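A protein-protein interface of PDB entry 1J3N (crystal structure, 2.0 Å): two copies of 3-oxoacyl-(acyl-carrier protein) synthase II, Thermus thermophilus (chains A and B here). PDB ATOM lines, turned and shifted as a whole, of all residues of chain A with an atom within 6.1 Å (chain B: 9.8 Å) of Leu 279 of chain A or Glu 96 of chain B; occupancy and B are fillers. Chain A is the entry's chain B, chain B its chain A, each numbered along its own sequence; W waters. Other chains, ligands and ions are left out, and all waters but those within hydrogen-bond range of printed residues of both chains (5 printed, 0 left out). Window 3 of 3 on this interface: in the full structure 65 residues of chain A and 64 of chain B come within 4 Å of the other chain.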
ATOM      1  N   GLY A 259      13.693  22.363 -18.109  1.00  0.00           N
ATOM      2  CA  GLY A 259      12.315  22.355 -17.644  1.00  0.00           C
ATOM      3  C   GLY A 259      11.312  22.634 -18.761  1.00  0.00           C
ATOM      4  O   GLY A 259      11.567  23.466 -19.630  1.00  0.00           O
ATOM      5  N   ARG A 260      10.182  21.922 -18.751  1.00  0.00           N
ATOM      6  CA  ARG A 260       9.137  22.094 -19.762  1.00  0.00           C
ATOM      7  C   ARG A 260       7.732  22.065 -19.164  1.00  0.00           C
ATOM      8  O   ARG A 260       7.504  21.491 -18.103  1.00  0.00           O
ATOM      9  CB  ARG A 260       9.235  21.004 -20.834  1.00  0.00           C
ATOM     10  CG  ARG A 260      10.429  21.123 -21.770  1.00  0.00           C
ATOM     11  CD  ARG A 260      10.419  19.981 -22.786  1.00  0.00           C
ATOM     12  NE  ARG A 260      10.585  18.685 -22.131  1.00  0.00           N
ATOM     13  CZ  ARG A 260      10.617  17.515 -22.767  1.00  0.00           C
ATOM     14  NH1 ARG A 260      10.496  17.470 -24.091  1.00  0.00           N
ATOM     15  NH2 ARG A 260      10.772  16.390 -22.077  1.00  0.00           N
ATOM     16  N   SER A 261       6.791  22.688 -19.864  1.00  0.00           N
ATOM     17  CA  SER A 261       5.402  22.728 -19.433  1.00  0.00           C
ATOM     18  C   SER A 261       4.563  23.184 -20.614  1.00  0.00           C
ATOM     19  O   SER A 261       5.099  23.521 -21.663  1.00  0.00           O
ATOM     20  CB  SER A 261       5.215  23.716 -18.286  1.00  0.00           C
ATOM     21  OG  SER A 261       5.382  25.046 -18.750  1.00  0.00           O
ATOM     22  N   ALA A 262       3.245  23.189 -20.431  1.00  0.00           N
ATOM     23  CA  ALA A 262       2.319  23.613 -21.475  1.00  0.00           C
ATOM     24  C   ALA A 262       1.316  24.580 -20.872  1.00  0.00           C
ATOM     25  O   ALA A 262       0.801  24.327 -19.792  1.00  0.00           O
ATOM     26  CB  ALA A 262       1.591  22.401 -22.049  1.00  0.00           C
ATOM     27  N   GLY A 274       1.755  34.395 -17.287  1.00  0.00           N
ATOM     28  CA  GLY A 274       2.973  33.606 -17.381  1.00  0.00           C
ATOM     29  C   GLY A 274       2.975  32.370 -16.500  1.00  0.00           C
ATOM     30  O   GLY A 274       4.020  31.962 -15.983  1.00  0.00           O
ATOM     31  N   LYS A 275       1.803  31.765 -16.342  1.00  0.00           N
ATOM     32  CA  LYS A 275       1.650  30.575 -15.516  1.00  0.00           C
ATOM     33  C   LYS A 275       2.464  29.387 -16.031  1.00  0.00           C
ATOM     34  O   LYS A 275       3.110  28.686 -15.255  1.00  0.00           O
ATOM     35  CB  LYS A 275       0.172  30.193 -15.442  1.00  0.00           C
ATOM     36  CG  LYS A 275      -0.129  28.978 -14.587  1.00  0.00           C
ATOM     37  CD  LYS A 275      -1.606  28.633 -14.690  1.00  0.00           C
ATOM     38  CE  LYS A 275      -1.972  27.448 -13.821  1.00  0.00           C
ATOM     39  NZ  LYS A 275      -3.434  27.162 -13.919  1.00  0.00           N
ATOM     40  N   GLY A 276       2.421  29.158 -17.338  1.00  0.00           N
ATOM     41  CA  GLY A 276       3.168  28.053 -17.912  1.00  0.00           C
ATOM     42  C   GLY A 276       4.656  28.345 -17.908  1.00  0.00           C
ATOM     43  O   GLY A 276       5.471  27.465 -17.625  1.00  0.00           O
ATOM     44  N   ALA A 277       4.997  29.587 -18.230  1.00  0.00           N
ATOM     45  CA  ALA A 277       6.382  30.028 -18.268  1.00  0.00           C
ATOM     46  C   ALA A 277       7.029  29.874 -16.896  1.00  0.00           C
ATOM     47  O   ALA A 277       8.166  29.422 -16.785  1.00  0.00           O
ATOM     48  CB  ALA A 277       6.455  31.488 -18.725  1.00  0.00           C
ATOM     49  N   ALA A 278       6.294  30.243 -15.854  1.00  0.00           N
ATOM     50  CA  ALA A 278       6.794  30.152 -14.485  1.00  0.00           C
ATOM     51  C   ALA A 278       7.039  28.705 -14.075  1.00  0.00           C
ATOM     52  O   ALA A 278       8.043  28.389 -13.436  1.00  0.00           O
ATOM     53  CB  ALA A 278       5.802  30.803 -13.530  1.00  0.00           C
ATOM     54  N   LEU A 279       6.114  27.825 -14.441  1.00  0.00           N
ATOM     55  CA  LEU A 279       6.236  26.415 -14.111  1.00  0.00           C
ATOM     56  C   LEU A 279       7.472  25.812 -14.776  1.00  0.00           C
ATOM     57  O   LEU A 279       8.218  25.054 -14.151  1.00  0.00           O
ATOM     58  CB  LEU A 279       4.970  25.673 -14.543  1.00  0.00           C
ATOM     59  CG  LEU A 279       4.895  24.163 -14.312  1.00  0.00           C
ATOM     60  CD1 LEU A 279       5.225  23.832 -12.865  1.00  0.00           C
ATOM     61  CD2 LEU A 279       3.497  23.674 -14.684  1.00  0.00           C
ATOM     62  N   ALA A 280       7.693  26.165 -16.039  1.00  0.00           N
ATOM     63  CA  ALA A 280       8.846  25.666 -16.787  1.00  0.00           C
ATOM     64  C   ALA A 280      10.147  26.127 -16.125  1.00  0.00           C
ATOM     65  O   ALA A 280      11.081  25.339 -15.955  1.00  0.00           O
ATOM     66  CB  ALA A 280       8.784  26.166 -18.220  1.00  0.00           C
ATOM     67  N   MET A 281      10.209  27.402 -15.756  1.00  0.00           N
ATOM     68  CA  MET A 281      11.400  27.930 -15.110  1.00  0.00           C
ATOM     69  C   MET A 281      11.656  27.200 -13.801  1.00  0.00           C
ATOM     70  O   MET A 281      12.793  26.832 -13.500  1.00  0.00           O
ATOM     71  CB  MET A 281      11.268  29.439 -14.866  1.00  0.00           C
ATOM     72  CG  MET A 281      11.429  30.267 -16.127  1.00  0.00           C
ATOM     73  SD  MET A 281      11.709  32.023 -15.832  1.00  0.00           S
ATOM     74  CE  MET A 281      10.013  32.645 -15.825  1.00  0.00           C
ATOM     75  N   ALA A 282      10.599  26.975 -13.028  1.00  0.00           N
ATOM     76  CA  ALA A 282      10.736  26.275 -11.757  1.00  0.00           C
ATOM     77  C   ALA A 282      11.239  24.852 -11.983  1.00  0.00           C
ATOM     78  O   ALA A 282      12.057  24.342 -11.222  1.00  0.00           O
ATOM     79  CB  ALA A 282       9.396  26.247 -11.023  1.00  0.00           C
ATOM     80  N   ARG A 283      10.752  24.212 -13.038  1.00  0.00           N
ATOM     81  CA  ARG A 283      11.159  22.848 -13.333  1.00  0.00           C
ATOM     82  C   ARG A 283      12.610  22.744 -13.756  1.00  0.00           C
ATOM     83  O   ARG A 283      13.299  21.793 -13.386  1.00  0.00           O
ATOM     84  CB  ARG A 283      10.247  22.258 -14.400  1.00  0.00           C
ATOM     85  CG  ARG A 283       8.895  21.910 -13.838  1.00  0.00           C
ATOM     86  CD  ARG A 283       7.876  21.586 -14.907  1.00  0.00           C
ATOM     87  NE  ARG A 283       6.716  20.961 -14.284  1.00  0.00           N
ATOM     88  CZ  ARG A 283       5.572  20.692 -14.904  1.00  0.00           C
ATOM     89  NH1 ARG A 283       5.410  20.992 -16.186  1.00  0.00           N
ATOM     90  NH2 ARG A 283       4.590  20.115 -14.229  1.00  0.00           N
ATOM     91  N   ALA A 284      13.079  23.719 -14.526  1.00  0.00           N
ATOM     92  CA  ALA A 284      14.463  23.712 -14.972  1.00  0.00           C
ATOM     93  C   ALA A 284      15.395  23.790 -13.760  1.00  0.00           C
ATOM     94  O   ALA A 284      16.387  23.063 -13.686  1.00  0.00           O
ATOM     95  CB  ALA A 284      14.717  24.879 -15.906  1.00  0.00           C
ATOM     96  N   ARG A 318       7.164  35.859 -10.365  1.00  0.00           N
ATOM     97  CA  ARG A 318       6.534  34.798  -9.589  1.00  0.00           C
ATOM     98  C   ARG A 318       7.551  33.752  -9.125  1.00  0.00           C
ATOM     99  O   ARG A 318       7.545  33.351  -7.968  1.00  0.00           O
ATOM    100  CB  ARG A 318       5.424  34.129 -10.409  1.00  0.00           C
ATOM    101  CG  ARG A 318       4.207  35.033 -10.642  1.00  0.00           C
ATOM    102  CD  ARG A 318       3.295  34.562 -11.783  1.00  0.00           C
ATOM    103  NE  ARG A 318       2.306  33.562 -11.381  1.00  0.00           N
ATOM    104  CZ  ARG A 318       2.585  32.298 -11.080  1.00  0.00           C
ATOM    105  NH1 ARG A 318       3.831  31.852 -11.131  1.00  0.00           N
ATOM    106  NH2 ARG A 318       1.609  31.472 -10.735  1.00  0.00           N
ATOM    107  N   PRO B  90      -9.550  13.508 -16.868  1.00  0.00           N
ATOM    108  CA  PRO B  90      -8.618  14.599 -16.563  1.00  0.00           C
ATOM    109  C   PRO B  90      -8.655  15.082 -15.116  1.00  0.00           C
ATOM    110  O   PRO B  90      -7.618  15.380 -14.524  1.00  0.00           O
ATOM    111  CB  PRO B  90      -9.005  15.691 -17.571  1.00  0.00           C
ATOM    112  CG  PRO B  90     -10.397  15.301 -18.030  1.00  0.00           C
ATOM    113  CD  PRO B  90     -10.320  13.809 -18.086  1.00  0.00           C
ATOM    114  N   GLU B  91      -9.854  15.140 -14.547  1.00  0.00           N
ATOM    115  CA  GLU B  91     -10.041  15.584 -13.171  1.00  0.00           C
ATOM    116  C   GLU B  91      -9.378  14.656 -12.154  1.00  0.00           C
ATOM    117  O   GLU B  91      -8.840  15.109 -11.145  1.00  0.00           O
ATOM    118  CB  GLU B  91     -11.537  15.702 -12.864  1.00  0.00           C
ATOM    119  CG  GLU B  91     -12.381  14.571 -13.446  1.00  0.00           C
ATOM    120  CD  GLU B  91     -12.605  14.714 -14.946  1.00  0.00           C
ATOM    121  OE1 GLU B  91     -11.947  15.568 -15.576  1.00  0.00           O
ATOM    122  OE2 GLU B  91     -13.438  13.967 -15.500  1.00  0.00           O
ATOM    123  N   ASP B  92      -9.419  13.356 -12.427  1.00  0.00           N
ATOM    124  CA  ASP B  92      -8.832  12.359 -11.538  1.00  0.00           C
ATOM    125  C   ASP B  92      -7.314  12.243 -11.727  1.00  0.00           C
ATOM    126  O   ASP B  92      -6.672  11.322 -11.208  1.00  0.00           O
ATOM    127  CB  ASP B  92      -9.507  11.013 -11.788  1.00  0.00           C
ATOM    128  CG  ASP B  92     -11.005  11.072 -11.559  1.00  0.00           C
ATOM    129  OD1 ASP B  92     -11.619  12.105 -11.910  1.00  0.00           O
ATOM    130  OD2 ASP B  92     -11.572  10.090 -11.039  1.00  0.00           O
ATOM    131  N   LEU B  93      -6.752  13.191 -12.470  1.00  0.00           N
ATOM    132  CA  LEU B  93      -5.320  13.230 -12.747  1.00  0.00           C
ATOM    133  C   LEU B  93      -4.754  14.594 -12.388  1.00  0.00           C
ATOM    134  O   LEU B  93      -5.412  15.614 -12.582  1.00  0.00           O
ATOM    135  CB  LEU B  93      -5.050  12.987 -14.232  1.00  0.00           C
ATOM    136  CG  LEU B  93      -5.350  11.622 -14.836  1.00  0.00           C
ATOM    137  CD1 LEU B  93      -5.056  11.670 -16.327  1.00  0.00           C
ATOM    138  CD2 LEU B  93      -4.504  10.559 -14.149  1.00  0.00           C
ATOM    139  N   ASP B  94      -3.534  14.613 -11.866  1.00  0.00           N
ATOM    140  CA  ASP B  94      -2.898  15.879 -11.536  1.00  0.00           C
ATOM    141  C   ASP B  94      -2.429  16.416 -12.891  1.00  0.00           C
ATOM    142  O   ASP B  94      -1.489  15.890 -13.489  1.00  0.00           O
ATOM    143  CB  ASP B  94      -1.718  15.648 -10.587  1.00  0.00           C
ATOM    144  CG  ASP B  94      -0.997  16.927 -10.237  1.00  0.00           C
ATOM    145  OD1 ASP B  94      -0.190  16.913  -9.285  1.00  0.00           O
ATOM    146  OD2 ASP B  94      -1.228  17.948 -10.917  1.00  0.00           O
ATOM    147  N   PRO B  95      -3.092  17.466 -13.397  1.00  0.00           N
ATOM    148  CA  PRO B  95      -2.748  18.064 -14.691  1.00  0.00           C
ATOM    149  C   PRO B  95      -1.285  18.436 -14.903  1.00  0.00           C
ATOM    150  O   PRO B  95      -0.798  18.412 -16.033  1.00  0.00           O
ATOM    151  CB  PRO B  95      -3.684  19.270 -14.772  1.00  0.00           C
ATOM    152  CG  PRO B  95      -3.888  19.638 -13.327  1.00  0.00           C
ATOM    153  CD  PRO B  95      -4.081  18.295 -12.684  1.00  0.00           C
ATOM    154  N   GLU B  96      -0.584  18.777 -13.826  1.00  0.00           N
ATOM    155  CA  GLU B  96       0.819  19.151 -13.927  1.00  0.00           C
ATOM    156  C   GLU B  96       1.716  17.947 -14.147  1.00  0.00           C
ATOM    157  O   GLU B  96       2.868  18.098 -14.547  1.00  0.00           O
ATOM    158  CB  GLU B  96       1.294  19.863 -12.657  1.00  0.00           C
ATOM    159  CG  GLU B  96       0.543  21.130 -12.322  1.00  0.00           C
ATOM    160  CD  GLU B  96       1.274  21.967 -11.289  1.00  0.00           C
ATOM    161  OE1 GLU B  96       1.789  21.391 -10.307  1.00  0.00           O
ATOM    162  OE2 GLU B  96       1.328  23.205 -11.457  1.00  0.00           O
ATOM    163  N   ARG B  97       1.185  16.760 -13.885  1.00  0.00           N
ATOM    164  CA  ARG B  97       1.964  15.537 -14.018  1.00  0.00           C
ATOM    165  C   ARG B  97       1.626  14.741 -15.269  1.00  0.00           C
ATOM    166  O   ARG B  97       2.103  13.618 -15.452  1.00  0.00           O
ATOM    167  CB  ARG B  97       1.771  14.679 -12.765  1.00  0.00           C
ATOM    168  CG  ARG B  97       2.159  15.405 -11.472  1.00  0.00           C
ATOM    169  CD  ARG B  97       3.616  15.825 -11.515  1.00  0.00           C
ATOM    170  NE  ARG B  97       4.483  14.674 -11.752  1.00  0.00           N
ATOM    171  CZ  ARG B  97       5.763  14.752 -12.102  1.00  0.00           C
ATOM    172  NH1 ARG B  97       6.346  15.935 -12.265  1.00  0.00           N
ATOM    173  NH2 ARG B  97       6.464  13.640 -12.277  1.00  0.00           N
ATOM    174  N   VAL B  98       0.801  15.328 -16.129  1.00  0.00           N
ATOM    175  CA  VAL B  98       0.412  14.679 -17.369  1.00  0.00           C
ATOM    176  C   VAL B  98       1.042  15.398 -18.547  1.00  0.00           C
ATOM    177  O   VAL B  98       0.843  16.599 -18.735  1.00  0.00           O
ATOM    178  CB  VAL B  98      -1.111  14.672 -17.567  1.00  0.00           C
ATOM    179  CG1 VAL B  98      -1.447  14.016 -18.902  1.00  0.00           C
ATOM    180  CG2 VAL B  98      -1.778  13.911 -16.433  1.00  0.00           C
ATOM    181  N   GLY B  99       1.804  14.648 -19.335  1.00  0.00           N
ATOM    182  CA  GLY B  99       2.458  15.217 -20.495  1.00  0.00           C
ATOM    183  C   GLY B  99       1.786  14.771 -21.775  1.00  0.00           C
ATOM    184  O   GLY B  99       0.951  13.857 -21.774  1.00  0.00           O
ATOM    185  N   THR B 100       2.153  15.425 -22.871  1.00  0.00           N
ATOM    186  CA  THR B 100       1.602  15.123 -24.181  1.00  0.00           C
ATOM    187  C   THR B 100       2.746  15.081 -25.195  1.00  0.00           C
ATOM    188  O   THR B 100       3.642  15.929 -25.171  1.00  0.00           O
ATOM    189  CB  THR B 100       0.564  16.193 -24.605  1.00  0.00           C
ATOM    190  OG1 THR B 100       1.145  17.490 -24.494  1.00  0.00           O
ATOM    191  CG2 THR B 100      -0.662  16.150 -23.714  1.00  0.00           C
ATOM    192  N   ALA B 145      -3.204  18.991 -24.972  1.00  0.00           N
ATOM    193  CA  ALA B 145      -2.884  19.612 -23.689  1.00  0.00           C
ATOM    194  C   ALA B 145      -3.922  20.668 -23.321  1.00  0.00           C
ATOM    195  O   ALA B 145      -4.321  20.785 -22.155  1.00  0.00           O
ATOM    196  CB  ALA B 145      -1.501  20.251 -23.744  1.00  0.00           C
ATOM    197  N   TYR B 148      -7.598  19.112 -22.314  1.00  0.00           N
ATOM    198  CA  TYR B 148      -7.673  18.495 -20.993  1.00  0.00           C
ATOM    199  C   TYR B 148      -6.971  19.248 -19.863  1.00  0.00           C
ATOM    200  O   TYR B 148      -7.063  18.851 -18.707  1.00  0.00           O
ATOM    201  CB  TYR B 148      -7.124  17.067 -21.065  1.00  0.00           C
ATOM    202  CG  TYR B 148      -7.852  16.181 -22.054  1.00  0.00           C
ATOM    203  CD1 TYR B 148      -9.206  15.876 -21.889  1.00  0.00           C
ATOM    204  CD2 TYR B 148      -7.191  15.650 -23.155  1.00  0.00           C
ATOM    205  CE1 TYR B 148      -9.877  15.063 -22.805  1.00  0.00           C
ATOM    206  CE2 TYR B 148      -7.850  14.840 -24.070  1.00  0.00           C
ATOM    207  CZ  TYR B 148      -9.191  14.549 -23.891  1.00  0.00           C
ATOM    208  OH  TYR B 148      -9.837  13.744 -24.803  1.00  0.00           O
ATOM    209  N   GLY B 149      -6.273  20.325 -20.194  1.00  0.00           N
ATOM    210  CA  GLY B 149      -5.581  21.100 -19.178  1.00  0.00           C
ATOM    211  C   GLY B 149      -4.322  20.442 -18.636  1.00  0.00           C
ATOM    212  O   GLY B 149      -3.909  20.729 -17.514  1.00  0.00           O
ATOM    213  N   PHE B 150      -3.717  19.555 -19.425  1.00  0.00           N
ATOM    214  CA  PHE B 150      -2.497  18.867 -19.015  1.00  0.00           C
ATOM    215  C   PHE B 150      -1.342  19.849 -19.147  1.00  0.00           C
ATOM    216  O   PHE B 150      -1.008  20.278 -20.254  1.00  0.00           O
ATOM    217  CB  PHE B 150      -2.241  17.646 -19.905  1.00  0.00           C
ATOM    218  CG  PHE B 150      -3.337  16.604 -19.868  1.00  0.00           C
ATOM    219  CD1 PHE B 150      -4.050  16.355 -18.699  1.00  0.00           C
ATOM    220  CD2 PHE B 150      -3.593  15.813 -20.985  1.00  0.00           C
ATOM    221  CE1 PHE B 150      -4.993  15.342 -18.633  1.00  0.00           C
ATOM    222  CE2 PHE B 150      -4.535  14.788 -20.939  1.00  0.00           C
ATOM    223  CZ  PHE B 150      -5.240  14.547 -19.760  1.00  0.00           C
ATOM    224  N   THR B 151      -0.725  20.213 -18.025  1.00  0.00           N
ATOM    225  CA  THR B 151       0.364  21.183 -18.061  1.00  0.00           C
ATOM    226  C   THR B 151       1.771  20.598 -17.919  1.00  0.00           C
ATOM    227  O   THR B 151       2.739  21.331 -17.663  1.00  0.00           O
ATOM    228  CB  THR B 151       0.171  22.271 -16.985  1.00  0.00           C
ATOM    229  OG1 THR B 151       0.149  21.657 -15.694  1.00  0.00           O
ATOM    230  CG2 THR B 151      -1.146  23.023 -17.213  1.00  0.00           C
ATOM    231  N   GLY B 152       1.875  19.282 -18.058  1.00  0.00           N
ATOM    232  CA  GLY B 152       3.172  18.634 -18.011  1.00  0.00           C
ATOM    233  C   GLY B 152       3.843  18.907 -19.352  1.00  0.00           C
ATOM    234  O   GLY B 152       3.206  19.471 -20.255  1.00  0.00           O
ATOM    235  N   PRO B 153       5.118  18.526 -19.532  1.00  0.00           N
ATOM    236  CA  PRO B 153       5.817  18.762 -20.802  1.00  0.00           C
ATOM    237  C   PRO B 153       4.973  18.418 -22.037  1.00  0.00           C
ATOM    238  O   PRO B 153       4.325  17.373 -22.079  1.00  0.00           O
ATOM    239  CB  PRO B 153       7.049  17.871 -20.676  1.00  0.00           C
ATOM    240  CG  PRO B 153       7.372  17.983 -19.218  1.00  0.00           C
ATOM    241  CD  PRO B 153       6.001  17.849 -18.564  1.00  0.00           C
ATOM    242  N   SER B 154       4.985  19.304 -23.030  1.00  0.00           N
ATOM    243  CA  SER B 154       4.224  19.119 -24.265  1.00  0.00           C
ATOM    244  C   SER B 154       5.187  19.242 -25.442  1.00  0.00           C
ATOM    245  O   SER B 154       5.519  20.349 -25.870  1.00  0.00           O
ATOM    246  CB  SER B 154       3.128  20.191 -24.368  1.00  0.00           C
ATOM    247  OG  SER B 154       2.232  19.927 -25.433  1.00  0.00           O
ATOM    248  N   MET B 174      10.632  10.532 -20.555  1.00  0.00           N
ATOM    249  CA  MET B 174       9.987  11.581 -19.792  1.00  0.00           C
ATOM    250  C   MET B 174       9.468  11.043 -18.451  1.00  0.00           C
ATOM    251  O   MET B 174       9.600  11.697 -17.412  1.00  0.00           O
ATOM    252  CB  MET B 174       8.835  12.128 -20.630  1.00  0.00           C
ATOM    253  CG  MET B 174       8.343  13.513 -20.297  1.00  0.00           C
ATOM    254  SD  MET B 174       7.027  13.918 -21.495  1.00  0.00           S
ATOM    255  CE  MET B 174       7.969  14.513 -22.864  1.00  0.00           C
ATOM    256  N   GLY B 178      11.228  11.221 -14.450  1.00  0.00           N
ATOM    257  CA  GLY B 178      10.441  11.932 -13.454  1.00  0.00           C
ATOM    258  C   GLY B 178       9.831  13.254 -13.902  1.00  0.00           C
ATOM    259  O   GLY B 178       9.359  14.031 -13.066  1.00  0.00           O
ATOM    260  N   GLU B 179       9.820  13.513 -15.209  1.00  0.00           N
ATOM    261  CA  GLU B 179       9.261  14.762 -15.738  1.00  0.00           C
ATOM    262  C   GLU B 179       7.738  14.698 -15.829  1.00  0.00           C
ATOM    263  O   GLU B 179       7.067  15.717 -15.999  1.00  0.00           O
ATOM    264  CB  GLU B 179       9.844  15.071 -17.128  1.00  0.00           C
ATOM    265  CG  GLU B 179      11.374  15.126 -17.160  1.00  0.00           C
ATOM    266  CD  GLU B 179      11.934  15.364 -18.553  1.00  0.00           C
ATOM    267  OE1 GLU B 179      11.473  14.695 -19.503  1.00  0.00           O
ATOM    268  OE2 GLU B 179      12.842  16.210 -18.703  1.00  0.00           O
ATOM    269  N   ALA B 180       7.200  13.491 -15.713  1.00  0.00           N
ATOM    270  CA  ALA B 180       5.763  13.276 -15.781  1.00  0.00           C
ATOM    271  C   ALA B 180       5.451  11.889 -15.245  1.00  0.00           C
ATOM    272  O   ALA B 180       6.327  11.022 -15.202  1.00  0.00           O
ATOM    273  CB  ALA B 180       5.280  13.400 -17.239  1.00  0.00           C
ATOM    274  N   ASP B 181       4.204  11.679 -14.833  1.00  0.00           N
ATOM    275  CA  ASP B 181       3.788  10.380 -14.318  1.00  0.00           C
ATOM    276  C   ASP B 181       2.919   9.650 -15.324  1.00  0.00           C
ATOM    277  O   ASP B 181       2.837   8.424 -15.317  1.00  0.00           O
ATOM    278  CB  ASP B 181       3.042  10.554 -13.000  1.00  0.00           C
ATOM    279  CG  ASP B 181       3.882  11.262 -11.977  1.00  0.00           C
ATOM    280  OD1 ASP B 181       5.074  10.900 -11.882  1.00  0.00           O
ATOM    281  OD2 ASP B 181       3.367  12.167 -11.282  1.00  0.00           O
ATOM    282  N   LEU B 182       2.276  10.415 -16.195  1.00  0.00           N
ATOM    283  CA  LEU B 182       1.423   9.842 -17.223  1.00  0.00           C
ATOM    284  C   LEU B 182       1.599  10.689 -18.479  1.00  0.00           C
ATOM    285  O   LEU B 182       1.716  11.910 -18.396  1.00  0.00           O
ATOM    286  CB  LEU B 182      -0.035   9.855 -16.747  1.00  0.00           C
ATOM    287  CG  LEU B 182      -1.048   8.973 -17.482  1.00  0.00           C
ATOM    288  CD1 LEU B 182      -2.302   8.804 -16.644  1.00  0.00           C
ATOM    289  CD2 LEU B 182      -1.370   9.591 -18.837  1.00  0.00           C
ATOM    290  N   VAL B 183       1.633  10.045 -19.642  1.00  0.00           N
ATOM    291  CA  VAL B 183       1.794  10.772 -20.893  1.00  0.00           C
ATOM    292  C   VAL B 183       0.962  10.183 -22.034  1.00  0.00           C
ATOM    293  O   VAL B 183       0.913   8.968 -22.215  1.00  0.00           O
ATOM    294  CB  VAL B 183       3.285  10.798 -21.349  1.00  0.00           C
ATOM    295  CG1 VAL B 183       3.395  11.462 -22.729  1.00  0.00           C
ATOM    296  CG2 VAL B 183       4.145  11.557 -20.328  1.00  0.00           C
HETATM  297  O   HOH W   1      11.363  18.191 -19.488  1.00  0.00           O
HETATM  298  O   HOH W   2       5.327  18.948 -11.491  1.00  0.00           O
HETATM  299  O   HOH W   3       8.006  18.208 -15.668  1.00  0.00           O
HETATM  300  O   HOH W   4       6.623  21.506 -23.091  1.00  0.00           O
HETATM  301  O   HOH W   5      13.100  14.066 -21.498  1.00  0.00           O
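Water W1 lies within hydrogen-bond range of OE2 of Glu 179 of chain B (2.6 Å) and NE of Arg 260 of chain A (2.8 Å). Water W5 lies within hydrogen-bond range of OE1 of Glu 179 of chain B (2.7 Å) and NH2 of Arg 260 of chain A (3.3 Å). Water W3 lies within hydrogen-bond range of the backbone carbonyl oxygen of Glu 179 of chain B (2.7 Å) and the guanidinium group of Arg 283 of chain A (3.3 Å). Water W4 lies within hydrogen-bond range of the backbone NH (N) of Ser 154 of chain B (2.7 Å) and the backbone carbonyl oxygen (O) of Ser 261 of chain A (2.9 Å). Water W2 lies within hydrogen-bond range of NH2 of Arg 283 of chain A (3.1 Å) and NH1 of Arg 97 of chain B (3.3 Å).
No position is printed for both chains.
NH1 of Arg 283 of chain A is in hydrogen-bond range of O of Thr 151 of chain B, 3.1 Å away. The backbone carbonyl oxygen of Glu 96 of chain B sits at hydrogen-bond distance from the guanidinium group of Arg 283 of chain A. OE1 of Glu 179 of chain B is in salt-bridge range of NH2 of Arg 260 of chain A (3.2 Å). The backbone carbonyl oxygen (O) of Thr 151 of chain B lies within hydrogen-bond range of the backbone NH (N) of Ala 262 of chain A (3.4 Å).
Of the 26 printed residues of chain B, 8 touch a printed residue of chain A. Hydrophobic or aromatic side chains of chain B within 4 Å of the printed part of chain A: Pro 153 and Met 174. Among the printed residues, 15 pairs touch across the chains. Among the printed residues, Asp or Glu carboxylates within 4 Å of a Lys or Arg side-chain nitrogen of the other chain: Arg 260 of chain A with Glu 179 of chain B.
No residue of chain B comes within 4 Å of Gly 276 of chain A. Ala 277 of chain A touches none of the printed residues of chain B. No residue of chain B comes within 4 Å of Ala 278 of chain A. No residue of chain B comes within 4 Å of Ala 280 of chain A. Printed residues of chain B within 4 Å of Arg 283 of chain A: Glu 96, Thr 151, Gly 152 and Pro 153. Of the printed residues of chain B, Ala 262 of chain A touches Phe 150 (3.8 Å), Thr 151 (3.4 Å), Gly 152 (3.7 Å) and Ser 154 (3.6 Å). Of the printed residues of chain B, Arg 260 of chain A touches Pro 153, Met 174 and Glu 179. Of the printed residues of chain A, Phe 150 of chain B touches Ala 262 (3.8 Å). Leu 93 of chain B touches none of the printed residues of chain A. The nearest residue of chain A that does not touch Glu 96 of chain B is Lys 275 of chain A (5.9 Å).
The backbone carbonyl oxygen (O) of Arg 260 of chain A lies within hydrogen-bond range of the guanidinium group (NH1) of Arg 283 of chain A. N of Thr 100 of chain B is in hydrogen-bond range of O of Pro 153 of chain B (3.0 Å). The backbone carbonyl oxygen of Gly 276 of chain A lies within hydrogen-bond range of the side-chain hydroxyl of Ser 261 of chain A, at 2.7 Å. The backbone carbonyl oxygen of Ala 145 of chain B lies within hydrogen-bond range of the backbone NH of Phe 150 of chain B (3.1 Å). O of Val 98 of chain B sits at hydrogen-bond distance from N of Gly 152 of chain B (3.0 Å).
Among the printed residues, pairs that only touch across the chains: Arg 260 of chain A with Pro 153 of chain B, Arg 260 of chain A with Met 174 of chain B, Ser 261 of chain A with Thr 151 of chain B, Ser 261 of chain A with Gly 152 of chain B, Ala 262 of chain A with Phe 150 of chain B, Ala 262 of chain A with Gly 152 of chain B, Ala 262 of chain A with Ser 154 of chain B, Leu 279 of chain A with Glu 96 of chain B, Leu 279 of chain A with Thr 151 of chain B, Arg 283 of chain A with Gly 152 of chain B and Arg 283 of chain A with Pro 153 of chain B.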
